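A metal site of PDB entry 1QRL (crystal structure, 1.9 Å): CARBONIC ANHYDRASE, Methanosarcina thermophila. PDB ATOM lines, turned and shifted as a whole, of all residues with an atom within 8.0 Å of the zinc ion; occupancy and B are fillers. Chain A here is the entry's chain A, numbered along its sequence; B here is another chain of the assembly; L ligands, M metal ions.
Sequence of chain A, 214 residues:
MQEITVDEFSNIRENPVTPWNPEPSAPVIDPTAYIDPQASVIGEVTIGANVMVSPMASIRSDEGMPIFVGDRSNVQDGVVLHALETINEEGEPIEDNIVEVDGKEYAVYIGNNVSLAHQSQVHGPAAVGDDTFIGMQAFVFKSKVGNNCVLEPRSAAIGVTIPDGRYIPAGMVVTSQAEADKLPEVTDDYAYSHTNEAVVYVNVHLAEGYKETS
NE2 of His 123 binds the zinc ion (2.2 Å). NE2 of His 118 of chain B binds the zinc ion. ND1 of His 82 binds the zinc ion, at 2.3 Å. The zinc ion is bound by an oxygen (O3) of the ligand (2.5 Å).
N of His 118 of chain B sits close to OE1 of Gln 76 of chain B, 3.2 Å away. OD1 of Asp 77 of chain B sits at hydrogen-bond distance from ND1 of His 118 of chain B. NE2 of Gln 121 is in hydrogen-bond range of O of His 118 of chain B (3.2 Å). The side-chain carboxylate (OD2) of Asp 62 sits at hydrogen-bond distance from a ring nitrogen (NE2) of His 82 (2.8 Å). The backbone NH of Gly 124 is in hydrogen-bond range of the backbone carbonyl oxygen of His 82 (2.8 Å). A ring nitrogen (NE2) of His 82 sits at hydrogen-bond distance from the guanidinium group (NH1) of Arg 60, at 3.4 Å.
Merely in contact with the zinc ion: Gln 76 of chain B (3.9 Å). Within 4 Å of the zinc ion: His 82, His 123, Gln 76 of chain B and His 118 of chain B.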
ATOM      1  N   ARG A  60     -21.741  -5.148  23.614  1.00  0.00           N
ATOM      2  CA  ARG A  60     -21.254  -6.344  24.296  1.00  0.00           C
ATOM      3  C   ARG A  60     -19.713  -6.378  24.226  1.00  0.00           C
ATOM      4  O   ARG A  60     -19.153  -6.516  23.169  1.00  0.00           O
ATOM      5  CB  ARG A  60     -21.900  -7.566  23.629  1.00  0.00           C
ATOM      6  CG  ARG A  60     -21.568  -8.952  24.219  1.00  0.00           C
ATOM      7  CD  ARG A  60     -22.603  -9.995  23.810  1.00  0.00           C
ATOM      8  NE  ARG A  60     -22.572 -10.338  22.361  1.00  0.00           N
ATOM      9  CZ  ARG A  60     -21.853 -11.306  21.784  1.00  0.00           C
ATOM     10  NH1 ARG A  60     -21.037 -12.052  22.549  1.00  0.00           N
ATOM     11  NH2 ARG A  60     -21.938 -11.525  20.447  1.00  0.00           N
ATOM     12  N   ASP A  62     -17.297  -8.560  25.653  1.00  0.00           N
ATOM     13  CA  ASP A  62     -17.006  -9.860  26.316  1.00  0.00           C
ATOM     14  C   ASP A  62     -15.929 -10.623  25.543  1.00  0.00           C
ATOM     15  O   ASP A  62     -15.471 -11.700  25.944  1.00  0.00           O
ATOM     16  CB  ASP A  62     -18.216 -10.799  26.414  1.00  0.00           C
ATOM     17  CG  ASP A  62     -18.871 -11.052  25.016  1.00  0.00           C
ATOM     18  OD1 ASP A  62     -19.971 -11.612  24.950  1.00  0.00           O
ATOM     19  OD2 ASP A  62     -18.328 -10.543  23.989  1.00  0.00           O
ATOM     20  N   GLU A  63     -15.449 -10.027  24.455  1.00  0.00           N
ATOM     21  CA  GLU A  63     -14.447 -10.731  23.606  1.00  0.00           C
ATOM     22  C   GLU A  63     -13.355  -9.675  23.518  1.00  0.00           C
ATOM     23  O   GLU A  63     -12.557  -9.577  24.482  1.00  0.00           O
ATOM     24  CB  GLU A  63     -15.078 -11.158  22.290  1.00  0.00           C
ATOM     25  CG  GLU A  63     -14.182 -11.945  21.347  1.00  0.00           C
ATOM     26  CD  GLU A  63     -14.732 -12.255  19.988  1.00  0.00           C
ATOM     27  OE1 GLU A  63     -15.962 -12.410  19.898  1.00  0.00           O
ATOM     28  OE2 GLU A  63     -14.024 -12.448  18.962  1.00  0.00           O
ATOM     29  N   GLY A  64     -13.434  -8.864  22.438  1.00  0.00           N
ATOM     30  CA  GLY A  64     -12.518  -7.712  22.397  1.00  0.00           C
ATOM     31  C   GLY A  64     -13.025  -6.702  23.453  1.00  0.00           C
ATOM     32  O   GLY A  64     -14.260  -6.547  23.663  1.00  0.00           O
ATOM     33  N   VAL A  80     -25.514  -2.635  17.036  1.00  0.00           N
ATOM     34  CA  VAL A  80     -24.664  -3.570  17.790  1.00  0.00           C
ATOM     35  C   VAL A  80     -23.222  -3.018  17.815  1.00  0.00           C
ATOM     36  O   VAL A  80     -22.646  -2.652  16.802  1.00  0.00           O
ATOM     37  CB  VAL A  80     -24.625  -4.928  17.070  1.00  0.00           C
ATOM     38  CG1 VAL A  80     -23.616  -5.850  17.770  1.00  0.00           C
ATOM     39  CG2 VAL A  80     -26.043  -5.542  17.171  1.00  0.00           C
ATOM     40  N   LEU A  81     -22.616  -3.105  19.000  1.00  0.00           N
ATOM     41  CA  LEU A  81     -21.193  -2.890  19.201  1.00  0.00           C
ATOM     42  C   LEU A  81     -20.614  -4.166  19.830  1.00  0.00           C
ATOM     43  O   LEU A  81     -21.034  -4.627  20.864  1.00  0.00           O
ATOM     44  CB  LEU A  81     -20.873  -1.796  20.264  1.00  0.00           C
ATOM     45  CG  LEU A  81     -21.517  -0.436  19.898  1.00  0.00           C
ATOM     46  CD1 LEU A  81     -21.143   0.634  20.948  1.00  0.00           C
ATOM     47  CD2 LEU A  81     -20.926   0.080  18.583  1.00  0.00           C
ATOM     48  N   HIS A  82     -19.581  -4.735  19.166  1.00  0.00           N
ATOM     49  CA  HIS A  82     -18.926  -5.944  19.611  1.00  0.00           C
ATOM     50  C   HIS A  82     -17.512  -5.988  19.031  1.00  0.00           C
ATOM     51  O   HIS A  82     -17.278  -5.120  18.166  1.00  0.00           O
ATOM     52  CB  HIS A  82     -19.670  -7.208  19.175  1.00  0.00           C
ATOM     53  CG  HIS A  82     -19.195  -8.414  19.926  1.00  0.00           C
ATOM     54  ND1 HIS A  82     -18.614  -9.444  19.309  1.00  0.00           N
ATOM     55  CD2 HIS A  82     -19.212  -8.816  21.215  1.00  0.00           C
ATOM     56  CE1 HIS A  82     -18.292 -10.533  20.063  1.00  0.00           C
ATOM     57  NE2 HIS A  82     -18.605 -10.074  21.288  1.00  0.00           N
ATOM     58  N   ALA A  83     -16.598  -6.887  19.491  1.00  0.00           N
ATOM     59  CA  ALA A  83     -15.287  -6.778  18.839  1.00  0.00           C
ATOM     60  C   ALA A  83     -14.496  -8.124  18.882  1.00  0.00           C
ATOM     61  O   ALA A  83     -14.830  -8.987  19.671  1.00  0.00           O
ATOM     62  CB  ALA A  83     -14.500  -5.802  19.735  1.00  0.00           C
ATOM     63  N   LEU A  84     -13.551  -8.199  17.956  1.00  0.00           N
ATOM     64  CA  LEU A  84     -12.685  -9.387  17.903  1.00  0.00           C
ATOM     65  C   LEU A  84     -11.818  -9.450  19.139  1.00  0.00           C
ATOM     66  O   LEU A  84     -11.548  -8.439  19.786  1.00  0.00           O
ATOM     67  CB  LEU A  84     -11.763  -9.344  16.648  1.00  0.00           C
ATOM     68  CG  LEU A  84     -12.534  -9.344  15.327  1.00  0.00           C
ATOM     69  CD1 LEU A  84     -11.627  -9.122  14.114  1.00  0.00           C
ATOM     70  CD2 LEU A  84     -13.373 -10.609  15.161  1.00  0.00           C
ATOM     71  N   GLU A  85     -11.389 -10.665  19.462  1.00  0.00           N
ATOM     72  CA  GLU A  85     -10.581 -10.918  20.669  1.00  0.00           C
ATOM     73  C   GLU A  85      -9.325 -10.051  20.702  1.00  0.00           C
ATOM     74  O   GLU A  85      -8.609  -9.863  19.697  1.00  0.00           O
ATOM     75  CB  GLU A  85     -10.305 -12.444  20.705  1.00  0.00           C
ATOM     76  CG  GLU A  85     -10.203 -12.978  22.134  1.00  0.00           C
ATOM     77  CD  GLU A  85      -9.568 -14.359  22.191  1.00  0.00           C
ATOM     78  OE1 GLU A  85      -9.873 -15.125  21.243  1.00  0.00           O
ATOM     79  OE2 GLU A  85      -8.784 -14.663  23.135  1.00  0.00           O
ATOM     80  N   GLN A 121     -23.908  -0.818  12.792  1.00  0.00           N
ATOM     81  CA  GLN A 121     -23.046  -1.680  13.626  1.00  0.00           C
ATOM     82  C   GLN A 121     -21.594  -1.186  13.494  1.00  0.00           C
ATOM     83  O   GLN A 121     -21.124  -0.985  12.357  1.00  0.00           O
ATOM     84  CB  GLN A 121     -23.094  -3.125  13.140  1.00  0.00           C
ATOM     85  CG  GLN A 121     -22.112  -4.124  13.817  1.00  0.00           C
ATOM     86  CD  GLN A 121     -22.248  -5.575  13.301  1.00  0.00           C
ATOM     87  OE1 GLN A 121     -21.338  -6.387  13.579  1.00  0.00           O
ATOM     88  NE2 GLN A 121     -23.311  -5.991  12.639  1.00  0.00           N
ATOM     89  N   VAL A 122     -20.875  -1.234  14.599  1.00  0.00           N
ATOM     90  CA  VAL A 122     -19.448  -0.910  14.593  1.00  0.00           C
ATOM     91  C   VAL A 122     -18.831  -2.080  15.286  1.00  0.00           C
ATOM     92  O   VAL A 122     -19.139  -2.356  16.482  1.00  0.00           O
ATOM     93  CB  VAL A 122     -19.163   0.412  15.303  1.00  0.00           C
ATOM     94  CG1 VAL A 122     -17.641   0.611  15.289  1.00  0.00           C
ATOM     95  CG2 VAL A 122     -19.900   1.609  14.686  1.00  0.00           C
ATOM     96  N   HIS A 123     -18.024  -2.843  14.552  1.00  0.00           N
ATOM     97  CA  HIS A 123     -17.394  -4.043  15.076  1.00  0.00           C
ATOM     98  C   HIS A 123     -15.872  -3.840  15.226  1.00  0.00           C
ATOM     99  O   HIS A 123     -15.206  -3.468  14.218  1.00  0.00           O
ATOM    100  CB  HIS A 123     -17.597  -5.178  14.039  1.00  0.00           C
ATOM    101  CG  HIS A 123     -17.337  -6.455  14.788  1.00  0.00           C
ATOM    102  ND1 HIS A 123     -16.045  -6.909  15.085  1.00  0.00           N
ATOM    103  CD2 HIS A 123     -18.270  -7.295  15.288  1.00  0.00           C
ATOM    104  CE1 HIS A 123     -16.166  -8.022  15.798  1.00  0.00           C
ATOM    105  NE2 HIS A 123     -17.471  -8.251  15.837  1.00  0.00           N
ATOM    106  N   GLY A 124     -15.367  -4.063  16.412  1.00  0.00           N
ATOM    107  CA  GLY A 124     -13.895  -3.833  16.584  1.00  0.00           C
ATOM    108  C   GLY A 124     -13.056  -4.912  15.898  1.00  0.00           C
ATOM    109  O   GLY A 124     -13.497  -6.013  15.596  1.00  0.00           O
ATOM    110  N   PHE A 141     -16.030  -1.870  10.311  1.00  0.00           N
ATOM    111  CA  PHE A 141     -15.290  -2.972  10.895  1.00  0.00           C
ATOM    112  C   PHE A 141     -13.796  -2.916  10.483  1.00  0.00           C
ATOM    113  O   PHE A 141     -13.518  -2.599   9.294  1.00  0.00           O
ATOM    114  CB  PHE A 141     -15.929  -4.274  10.381  1.00  0.00           C
ATOM    115  CG  PHE A 141     -15.185  -5.551  10.687  1.00  0.00           C
ATOM    116  CD1 PHE A 141     -14.717  -5.817  11.958  1.00  0.00           C
ATOM    117  CD2 PHE A 141     -15.006  -6.486   9.695  1.00  0.00           C
ATOM    118  CE1 PHE A 141     -14.064  -7.011  12.254  1.00  0.00           C
ATOM    119  CE2 PHE A 141     -14.384  -7.673   9.955  1.00  0.00           C
ATOM    120  CZ  PHE A 141     -13.900  -7.934  11.239  1.00  0.00           C
ATOM    121  N   GLN B  76     -25.597 -14.682  16.664  1.00  0.00           N
ATOM    122  CA  GLN B  76     -25.138 -13.438  17.273  1.00  0.00           C
ATOM    123  C   GLN B  76     -26.222 -12.373  17.421  1.00  0.00           C
ATOM    124  O   GLN B  76     -27.380 -12.541  17.163  1.00  0.00           O
ATOM    125  CB  GLN B  76     -23.862 -12.905  16.608  1.00  0.00           C
ATOM    126  CG  GLN B  76     -22.737 -13.977  16.790  1.00  0.00           C
ATOM    127  CD  GLN B  76     -21.504 -13.471  16.084  1.00  0.00           C
ATOM    128  OE1 GLN B  76     -21.256 -12.296  15.808  1.00  0.00           O
ATOM    129  NE2 GLN B  76     -20.619 -14.431  15.775  1.00  0.00           N
ATOM    130  N   ASP B  77     -25.802 -11.186  17.955  1.00  0.00           N
ATOM    131  CA  ASP B  77     -26.773 -10.228  18.400  1.00  0.00           C
ATOM    132  C   ASP B  77     -27.638  -9.748  17.232  1.00  0.00           C
ATOM    133  O   ASP B  77     -27.095  -9.467  16.155  1.00  0.00           O
ATOM    134  CB  ASP B  77     -26.109  -8.907  18.976  1.00  0.00           C
ATOM    135  CG  ASP B  77     -24.943  -9.295  19.894  1.00  0.00           C
ATOM    136  OD1 ASP B  77     -23.948  -9.827  19.384  1.00  0.00           O
ATOM    137  OD2 ASP B  77     -24.971  -9.023  21.114  1.00  0.00           O
ATOM    138  N   ALA B 117     -23.115 -14.217  12.201  1.00  0.00           N
ATOM    139  CA  ALA B 117     -22.563 -13.014  12.859  1.00  0.00           C
ATOM    140  C   ALA B 117     -23.569 -11.880  13.023  1.00  0.00           C
ATOM    141  O   ALA B 117     -24.675 -11.903  12.483  1.00  0.00           O
ATOM    142  CB  ALA B 117     -21.283 -12.668  12.159  1.00  0.00           C
ATOM    143  N   HIS B 118     -23.270 -10.863  13.822  1.00  0.00           N
ATOM    144  CA  HIS B 118     -24.242  -9.882  14.244  1.00  0.00           C
ATOM    145  C   HIS B 118     -25.115  -9.274  13.151  1.00  0.00           C
ATOM    146  O   HIS B 118     -24.573  -8.867  12.100  1.00  0.00           O
ATOM    147  CB  HIS B 118     -23.533  -8.671  14.947  1.00  0.00           C
ATOM    148  CG  HIS B 118     -22.431  -9.088  15.859  1.00  0.00           C
ATOM    149  ND1 HIS B 118     -22.657  -9.456  17.179  1.00  0.00           N
ATOM    150  CD2 HIS B 118     -21.084  -9.167  15.600  1.00  0.00           C
ATOM    151  CE1 HIS B 118     -21.507  -9.747  17.774  1.00  0.00           C
ATOM    152  NE2 HIS B 118     -20.638  -9.656  16.782  1.00  0.00           N
ATOM    153  N   PHE B 133     -18.979 -19.285   7.849  1.00  0.00           N
ATOM    154  CA  PHE B 133     -19.200 -18.020   8.552  1.00  0.00           C
ATOM    155  C   PHE B 133     -20.247 -17.234   7.777  1.00  0.00           C
ATOM    156  O   PHE B 133     -19.963 -16.918   6.609  1.00  0.00           O
ATOM    157  CB  PHE B 133     -17.847 -17.306   8.636  1.00  0.00           C
ATOM    158  CG  PHE B 133     -17.850 -15.931   9.285  1.00  0.00           C
ATOM    159  CD1 PHE B 133     -17.841 -15.830  10.686  1.00  0.00           C
ATOM    160  CD2 PHE B 133     -17.875 -14.769   8.554  1.00  0.00           C
ATOM    161  CE1 PHE B 133     -17.793 -14.566  11.281  1.00  0.00           C
ATOM    162  CE2 PHE B 133     -17.859 -13.501   9.150  1.00  0.00           C
ATOM    163  CZ  PHE B 133     -17.827 -13.438  10.547  1.00  0.00           C
ATOM    164  N   MET B 136     -21.415 -10.309   9.195  1.00  0.00           N
ATOM    165  CA  MET B 136     -22.239  -9.292   9.807  1.00  0.00           C
ATOM    166  C   MET B 136     -23.162  -8.696   8.768  1.00  0.00           C
ATOM    167  O   MET B 136     -22.734  -8.355   7.655  1.00  0.00           O
ATOM    168  CB  MET B 136     -21.395  -8.180  10.472  1.00  0.00           C
ATOM    169  CG  MET B 136     -20.345  -8.548  11.516  1.00  0.00           C
ATOM    170  SD  MET B 136     -18.814  -9.251  10.857  1.00  0.00           S
ATOM    171  CE  MET B 136     -17.896  -9.569  12.354  1.00  0.00           C
ATOM    172  N   VAL B 199     -14.014 -17.825  15.631  1.00  0.00           N
ATOM    173  CA  VAL B 199     -15.293 -17.369  16.161  1.00  0.00           C
ATOM    174  C   VAL B 199     -16.004 -18.507  16.913  1.00  0.00           C
ATOM    175  O   VAL B 199     -16.644 -18.271  17.949  1.00  0.00           O
ATOM    176  CB  VAL B 199     -16.180 -16.823  15.009  1.00  0.00           C
ATOM    177  CG1 VAL B 199     -17.561 -16.408  15.460  1.00  0.00           C
ATOM    178  CG2 VAL B 199     -15.425 -15.647  14.362  1.00  0.00           C
ATOM    179  N   VAL B 202     -14.229 -19.133  20.204  1.00  0.00           N
ATOM    180  CA  VAL B 202     -14.649 -18.056  21.143  1.00  0.00           C
ATOM    181  C   VAL B 202     -16.035 -18.275  21.653  1.00  0.00           C
ATOM    182  O   VAL B 202     -16.308 -18.127  22.850  1.00  0.00           O
ATOM    183  CB  VAL B 202     -14.503 -16.697  20.411  1.00  0.00           C
ATOM    184  CG1 VAL B 202     -15.187 -15.559  21.155  1.00  0.00           C
ATOM    185  CG2 VAL B 202     -13.031 -16.362  20.236  1.00  0.00           C
ATOM    186  N   ASN B 203     -17.043 -18.428  20.785  1.00  0.00           N
ATOM    187  CA  ASN B 203     -18.434 -18.580  21.159  1.00  0.00           C
ATOM    188  C   ASN B 203     -18.743 -19.805  21.949  1.00  0.00           C
ATOM    189  O   ASN B 203     -19.577 -19.791  22.866  1.00  0.00           O
ATOM    190  CB  ASN B 203     -19.396 -18.456  19.915  1.00  0.00           C
ATOM    191  CG  ASN B 203     -19.539 -16.970  19.491  1.00  0.00           C
ATOM    192  OD1 ASN B 203     -20.544 -16.372  19.952  1.00  0.00           O
ATOM    193  ND2 ASN B 203     -18.662 -16.396  18.700  1.00  0.00           N
ATOM    194  N   LEU B 206     -17.636 -18.592  25.282  1.00  0.00           N
ATOM    195  CA  LEU B 206     -18.582 -17.610  25.847  1.00  0.00           C
ATOM    196  C   LEU B 206     -19.833 -18.293  26.310  1.00  0.00           C
ATOM    197  O   LEU B 206     -20.418 -17.968  27.374  1.00  0.00           O
ATOM    198  CB  LEU B 206     -18.916 -16.493  24.836  1.00  0.00           C
ATOM    199  CG  LEU B 206     -17.926 -15.418  24.523  1.00  0.00           C
ATOM    200  CD1 LEU B 206     -18.349 -14.669  23.234  1.00  0.00           C
ATOM    201  CD2 LEU B 206     -17.848 -14.408  25.709  1.00  0.00           C
HETATM  202  C1  LIG L   1     -16.486 -12.288  16.887  1.00  0.00           C
HETATM  203  O1  LIG L   1     -17.402 -12.537  15.914  1.00  0.00           O
HETATM  204  O2  LIG L   1     -15.836 -13.239  17.441  1.00  0.00           O
HETATM  205  O3  LIG L   1     -16.287 -11.039  17.325  1.00  0.00           O
HETATM  206 ZN    ZN M   1     -18.431  -9.835  17.039  1.00  0.00          ZN
